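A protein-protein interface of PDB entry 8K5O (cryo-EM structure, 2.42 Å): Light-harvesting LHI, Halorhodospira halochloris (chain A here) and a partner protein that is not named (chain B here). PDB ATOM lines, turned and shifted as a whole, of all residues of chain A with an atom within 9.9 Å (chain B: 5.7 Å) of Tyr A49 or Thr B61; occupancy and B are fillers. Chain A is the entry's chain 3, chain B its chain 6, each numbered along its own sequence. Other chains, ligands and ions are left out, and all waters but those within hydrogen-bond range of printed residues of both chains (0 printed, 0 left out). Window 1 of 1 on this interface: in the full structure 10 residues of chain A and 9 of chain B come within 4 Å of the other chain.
Tyr A49 touches just these residues of chain B: Thr B61 (3.3 Å), Ser B62 (3.4 Å) and Tyr B63 (3.1 Å). Of the printed residues of chain B, Tyr A50 touches Tyr B63. Of the printed residues of chain B, Ser A51 touches Tyr B63. No residue of chain A comes within 4 Å of Lys B59. Of chain A, only Tyr A49 (3.3 Å) comes within 4 Å of Thr B61. Of the printed residues of chain A, Ser B62 touches Tyr A49. Of the printed residues of chain A, Tyr B63 touches Tyr A49 (3.1 Å), Tyr A50 (3.2 Å) and Ser A51 (3.3 Å). The nearest residue of chain B that does not touch Tyr A49 is Glu B53 (4.2 Å). The nearest printed residue of chain B that does not touch Tyr A50 is Ser B62 (5.3 Å).
The backbone carbonyl oxygen (O) of Tyr A49 is in hydrogen-bond range of the backbone NH (N) of Tyr B63, 3.1 Å away.
Of the 8 printed residues of chain B, 3 touch a printed residue of chain A. Hydrophobic or aromatic side chains of chain B that line the printed part of chain A: Tyr B63. Among the printed residues, 5 pairs touch across the chains.
Thr B61 touches Tyr A49 (O to CD1, 3.3 Å). Tyr A49 touches Ser B62. Tyr A50 touches Tyr B63 (O to CD2, 3.2 Å). O of Ser A51 touches CZ of Tyr B63, 3.3 Å away.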
ATOM      1  N   ARG A  37       9.518 -18.708 -38.330  1.00  0.00           N
ATOM      2  CA  ARG A  37       9.134 -19.184 -37.009  1.00  0.00           C
ATOM      3  C   ARG A  37       8.014 -20.205 -37.098  1.00  0.00           C
ATOM      4  O   ARG A  37       7.989 -21.179 -36.339  1.00  0.00           O
ATOM      5  CB  ARG A  37       8.695 -18.014 -36.143  1.00  0.00           C
ATOM      6  CG  ARG A  37       8.253 -18.411 -34.760  1.00  0.00           C
ATOM      7  CD  ARG A  37       7.687 -17.208 -34.118  1.00  0.00           C
ATOM      8  NE  ARG A  37       7.159 -17.345 -32.771  1.00  0.00           N
ATOM      9  CZ  ARG A  37       7.905 -17.350 -31.678  1.00  0.00           C
ATOM     10  NH1 ARG A  37       9.222 -17.257 -31.738  1.00  0.00           N
ATOM     11  NH2 ARG A  37       7.313 -17.424 -30.492  1.00  0.00           N
ATOM     12  N   ALA A  44      12.339 -24.406 -38.314  1.00  0.00           N
ATOM     13  CA  ALA A  44      13.367 -23.519 -37.796  1.00  0.00           C
ATOM     14  C   ALA A  44      13.189 -23.305 -36.293  1.00  0.00           C
ATOM     15  O   ALA A  44      12.079 -23.414 -35.771  1.00  0.00           O
ATOM     16  CB  ALA A  44      13.329 -22.180 -38.523  1.00  0.00           C
ATOM     17  N   PRO A  45      14.270 -23.004 -35.578  1.00  0.00           N
ATOM     18  CA  PRO A  45      14.158 -22.749 -34.139  1.00  0.00           C
ATOM     19  C   PRO A  45      13.386 -21.474 -33.846  1.00  0.00           C
ATOM     20  O   PRO A  45      13.264 -20.571 -34.675  1.00  0.00           O
ATOM     21  CB  PRO A  45      15.613 -22.620 -33.679  1.00  0.00           C
ATOM     22  CG  PRO A  45      16.435 -23.150 -34.791  1.00  0.00           C
ATOM     23  CD  PRO A  45      15.664 -22.940 -36.039  1.00  0.00           C
ATOM     24  N   ALA A  46      12.847 -21.420 -32.636  1.00  0.00           N
ATOM     25  CA  ALA A  46      12.163 -20.234 -32.154  1.00  0.00           C
ATOM     26  C   ALA A  46      13.138 -19.323 -31.419  1.00  0.00           C
ATOM     27  O   ALA A  46      14.119 -19.770 -30.822  1.00  0.00           O
ATOM     28  CB  ALA A  46      11.004 -20.612 -31.234  1.00  0.00           C
ATOM     29  N   ALA A  47      12.848 -18.024 -31.465  1.00  0.00           N
ATOM     30  CA  ALA A  47      13.698 -17.044 -30.803  1.00  0.00           C
ATOM     31  C   ALA A  47      13.688 -17.191 -29.289  1.00  0.00           C
ATOM     32  O   ALA A  47      14.639 -16.754 -28.636  1.00  0.00           O
ATOM     33  CB  ALA A  47      13.266 -15.634 -31.188  1.00  0.00           C
ATOM     34  N   GLU A  48      12.641 -17.787 -28.715  1.00  0.00           N
ATOM     35  CA  GLU A  48      12.606 -17.994 -27.271  1.00  0.00           C
ATOM     36  C   GLU A  48      13.691 -18.958 -26.818  1.00  0.00           C
ATOM     37  O   GLU A  48      14.136 -18.900 -25.667  1.00  0.00           O
ATOM     38  CB  GLU A  48      11.234 -18.516 -26.850  1.00  0.00           C
ATOM     39  CG  GLU A  48      10.132 -17.481 -26.891  1.00  0.00           C
ATOM     40  CD  GLU A  48       9.439 -17.426 -28.234  1.00  0.00           C
ATOM     41  OE1 GLU A  48      10.119 -17.598 -29.266  1.00  0.00           O
ATOM     42  OE2 GLU A  48       8.210 -17.208 -28.260  1.00  0.00           O
ATOM     43  N   TYR A  49      14.119 -19.854 -27.703  1.00  0.00           N
ATOM     44  CA  TYR A  49      15.178 -20.800 -27.398  1.00  0.00           C
ATOM     45  C   TYR A  49      16.559 -20.159 -27.404  1.00  0.00           C
ATOM     46  O   TYR A  49      17.447 -20.640 -26.692  1.00  0.00           O
ATOM     47  CB  TYR A  49      15.126 -21.946 -28.408  1.00  0.00           C
ATOM     48  CG  TYR A  49      16.052 -23.101 -28.125  1.00  0.00           C
ATOM     49  CD1 TYR A  49      15.689 -24.102 -27.239  1.00  0.00           C
ATOM     50  CD2 TYR A  49      17.272 -23.207 -28.766  1.00  0.00           C
ATOM     51  CE1 TYR A  49      16.528 -25.163 -26.986  1.00  0.00           C
ATOM     52  CE2 TYR A  49      18.117 -24.261 -28.521  1.00  0.00           C
ATOM     53  CZ  TYR A  49      17.742 -25.237 -27.630  1.00  0.00           C
ATOM     54  OH  TYR A  49      18.583 -26.295 -27.382  1.00  0.00           O
ATOM     55  N   TYR A  50      16.746 -19.078 -28.166  1.00  0.00           N
ATOM     56  CA  TYR A  50      18.059 -18.490 -28.430  1.00  0.00           C
ATOM     57  C   TYR A  50      18.992 -19.532 -29.050  1.00  0.00           C
ATOM     58  O   TYR A  50      20.062 -19.843 -28.524  1.00  0.00           O
ATOM     59  CB  TYR A  50      18.666 -17.889 -27.157  1.00  0.00           C
ATOM     60  CG  TYR A  50      17.662 -17.234 -26.243  1.00  0.00           C
ATOM     61  CD1 TYR A  50      16.852 -16.207 -26.694  1.00  0.00           C
ATOM     62  CD2 TYR A  50      17.521 -17.649 -24.925  1.00  0.00           C
ATOM     63  CE1 TYR A  50      15.928 -15.609 -25.863  1.00  0.00           C
ATOM     64  CE2 TYR A  50      16.600 -17.053 -24.086  1.00  0.00           C
ATOM     65  CZ  TYR A  50      15.807 -16.035 -24.563  1.00  0.00           C
ATOM     66  OH  TYR A  50      14.888 -15.435 -23.737  1.00  0.00           O
ATOM     67  N   SER A  51      18.557 -20.064 -30.189  1.00  0.00           N
ATOM     68  CA  SER A  51      19.163 -21.241 -30.815  1.00  0.00           C
ATOM     69  C   SER A  51      20.682 -21.229 -30.860  1.00  0.00           C
ATOM     70  O   SER A  51      21.309 -22.272 -31.035  1.00  0.00           O
ATOM     71  CB  SER A  51      18.630 -21.405 -32.235  1.00  0.00           C
ATOM     72  OG  SER A  51      18.971 -22.679 -32.751  1.00  0.00           O
ATOM     73  N   GLU B  53      18.714 -34.610 -26.150  1.00  0.00           N
ATOM     74  CA  GLU B  53      17.484 -34.303 -25.438  1.00  0.00           C
ATOM     75  C   GLU B  53      16.286 -34.327 -26.380  1.00  0.00           C
ATOM     76  O   GLU B  53      16.407 -34.090 -27.585  1.00  0.00           O
ATOM     77  CB  GLU B  53      17.588 -32.935 -24.761  1.00  0.00           C
ATOM     78  CG  GLU B  53      17.625 -31.763 -25.727  1.00  0.00           C
ATOM     79  CD  GLU B  53      19.025 -31.458 -26.227  1.00  0.00           C
ATOM     80  OE1 GLU B  53      19.918 -32.316 -26.067  1.00  0.00           O
ATOM     81  OE2 GLU B  53      19.232 -30.360 -26.783  1.00  0.00           O
ATOM     82  N   ASP B  54      15.128 -34.628 -25.815  1.00  0.00           N
ATOM     83  CA  ASP B  54      13.887 -34.553 -26.569  1.00  0.00           C
ATOM     84  C   ASP B  54      13.601 -33.100 -26.935  1.00  0.00           C
ATOM     85  O   ASP B  54      13.664 -32.225 -26.064  1.00  0.00           O
ATOM     86  CB  ASP B  54      12.742 -35.136 -25.744  1.00  0.00           C
ATOM     87  CG  ASP B  54      11.380 -34.852 -26.342  1.00  0.00           C
ATOM     88  OD1 ASP B  54      11.064 -35.414 -27.411  1.00  0.00           O
ATOM     89  OD2 ASP B  54      10.619 -34.073 -25.733  1.00  0.00           O
ATOM     90  N   PRO B  55      13.290 -32.797 -28.199  1.00  0.00           N
ATOM     91  CA  PRO B  55      12.968 -31.403 -28.530  1.00  0.00           C
ATOM     92  C   PRO B  55      11.641 -30.969 -27.949  1.00  0.00           C
ATOM     93  O   PRO B  55      11.521 -29.845 -27.448  1.00  0.00           O
ATOM     94  CB  PRO B  55      12.950 -31.394 -30.065  1.00  0.00           C
ATOM     95  CG  PRO B  55      12.873 -32.836 -30.489  1.00  0.00           C
ATOM     96  CD  PRO B  55      12.905 -33.718 -29.280  1.00  0.00           C
ATOM     97  N   LYS B  59       7.538 -27.264 -24.965  1.00  0.00           N
ATOM     98  CA  LYS B  59       8.407 -27.693 -23.876  1.00  0.00           C
ATOM     99  C   LYS B  59       9.136 -26.544 -23.196  1.00  0.00           C
ATOM    100  O   LYS B  59       9.723 -26.758 -22.129  1.00  0.00           O
ATOM    101  CB  LYS B  59       9.433 -28.709 -24.384  1.00  0.00           C
ATOM    102  CG  LYS B  59       9.917 -29.689 -23.324  1.00  0.00           C
ATOM    103  CD  LYS B  59      10.934 -30.668 -23.889  1.00  0.00           C
ATOM    104  CE  LYS B  59      12.034 -30.966 -22.886  1.00  0.00           C
ATOM    105  NZ  LYS B  59      13.101 -31.828 -23.468  1.00  0.00           N
ATOM    106  N   ARG B  60       9.104 -25.342 -23.771  1.00  0.00           N
ATOM    107  CA  ARG B  60       9.815 -24.188 -23.222  1.00  0.00           C
ATOM    108  C   ARG B  60      11.299 -24.496 -23.042  1.00  0.00           C
ATOM    109  O   ARG B  60      11.904 -24.160 -22.023  1.00  0.00           O
ATOM    110  CB  ARG B  60       9.190 -23.724 -21.905  1.00  0.00           C
ATOM    111  CG  ARG B  60       7.684 -23.562 -21.954  1.00  0.00           C
ATOM    112  CD  ARG B  60       7.250 -22.738 -23.152  1.00  0.00           C
ATOM    113  NE  ARG B  60       5.870 -22.290 -23.033  1.00  0.00           N
ATOM    114  CZ  ARG B  60       4.912 -22.588 -23.900  1.00  0.00           C
ATOM    115  NH1 ARG B  60       5.149 -23.343 -24.958  1.00  0.00           N
ATOM    116  NH2 ARG B  60       3.683 -22.120 -23.697  1.00  0.00           N
ATOM    117  N   THR B  61      11.884 -25.155 -24.038  1.00  0.00           N
ATOM    118  CA  THR B  61      13.292 -25.515 -23.979  1.00  0.00           C
ATOM    119  C   THR B  61      14.174 -24.279 -24.118  1.00  0.00           C
ATOM    120  O   THR B  61      13.783 -23.270 -24.712  1.00  0.00           O
ATOM    121  CB  THR B  61      13.635 -26.526 -25.074  1.00  0.00           C
ATOM    122  OG1 THR B  61      12.998 -26.146 -26.298  1.00  0.00           O
ATOM    123  CG2 THR B  61      13.171 -27.916 -24.680  1.00  0.00           C
ATOM    124  N   SER B  62      15.378 -24.369 -23.561  1.00  0.00           N
ATOM    125  CA  SER B  62      16.332 -23.272 -23.570  1.00  0.00           C
ATOM    126  C   SER B  62      17.677 -23.765 -24.082  1.00  0.00           C
ATOM    127  O   SER B  62      18.024 -24.940 -23.936  1.00  0.00           O
ATOM    128  CB  SER B  62      16.501 -22.663 -22.171  1.00  0.00           C
ATOM    129  OG  SER B  62      15.479 -21.721 -21.896  1.00  0.00           O
ATOM    130  N   TYR B  63      18.430 -22.855 -24.689  1.00  0.00           N
ATOM    131  CA  TYR B  63      19.755 -23.177 -25.201  1.00  0.00           C
ATOM    132  C   TYR B  63      20.729 -23.485 -24.067  1.00  0.00           C
ATOM    133  O   TYR B  63      20.687 -22.856 -23.011  1.00  0.00           O
ATOM    134  CB  TYR B  63      20.293 -22.028 -26.055  1.00  0.00           C
ATOM    135  CG  TYR B  63      21.416 -22.430 -26.980  1.00  0.00           C
ATOM    136  CD1 TYR B  63      21.427 -23.677 -27.586  1.00  0.00           C
ATOM    137  CD2 TYR B  63      22.468 -21.565 -27.242  1.00  0.00           C
ATOM    138  CE1 TYR B  63      22.451 -24.051 -28.431  1.00  0.00           C
ATOM    139  CE2 TYR B  63      23.496 -21.930 -28.088  1.00  0.00           C
ATOM    140  CZ  TYR B  63      23.483 -23.175 -28.679  1.00  0.00           C
ATOM    141  OH  TYR B  63      24.506 -23.546 -29.522  1.00  0.00           O
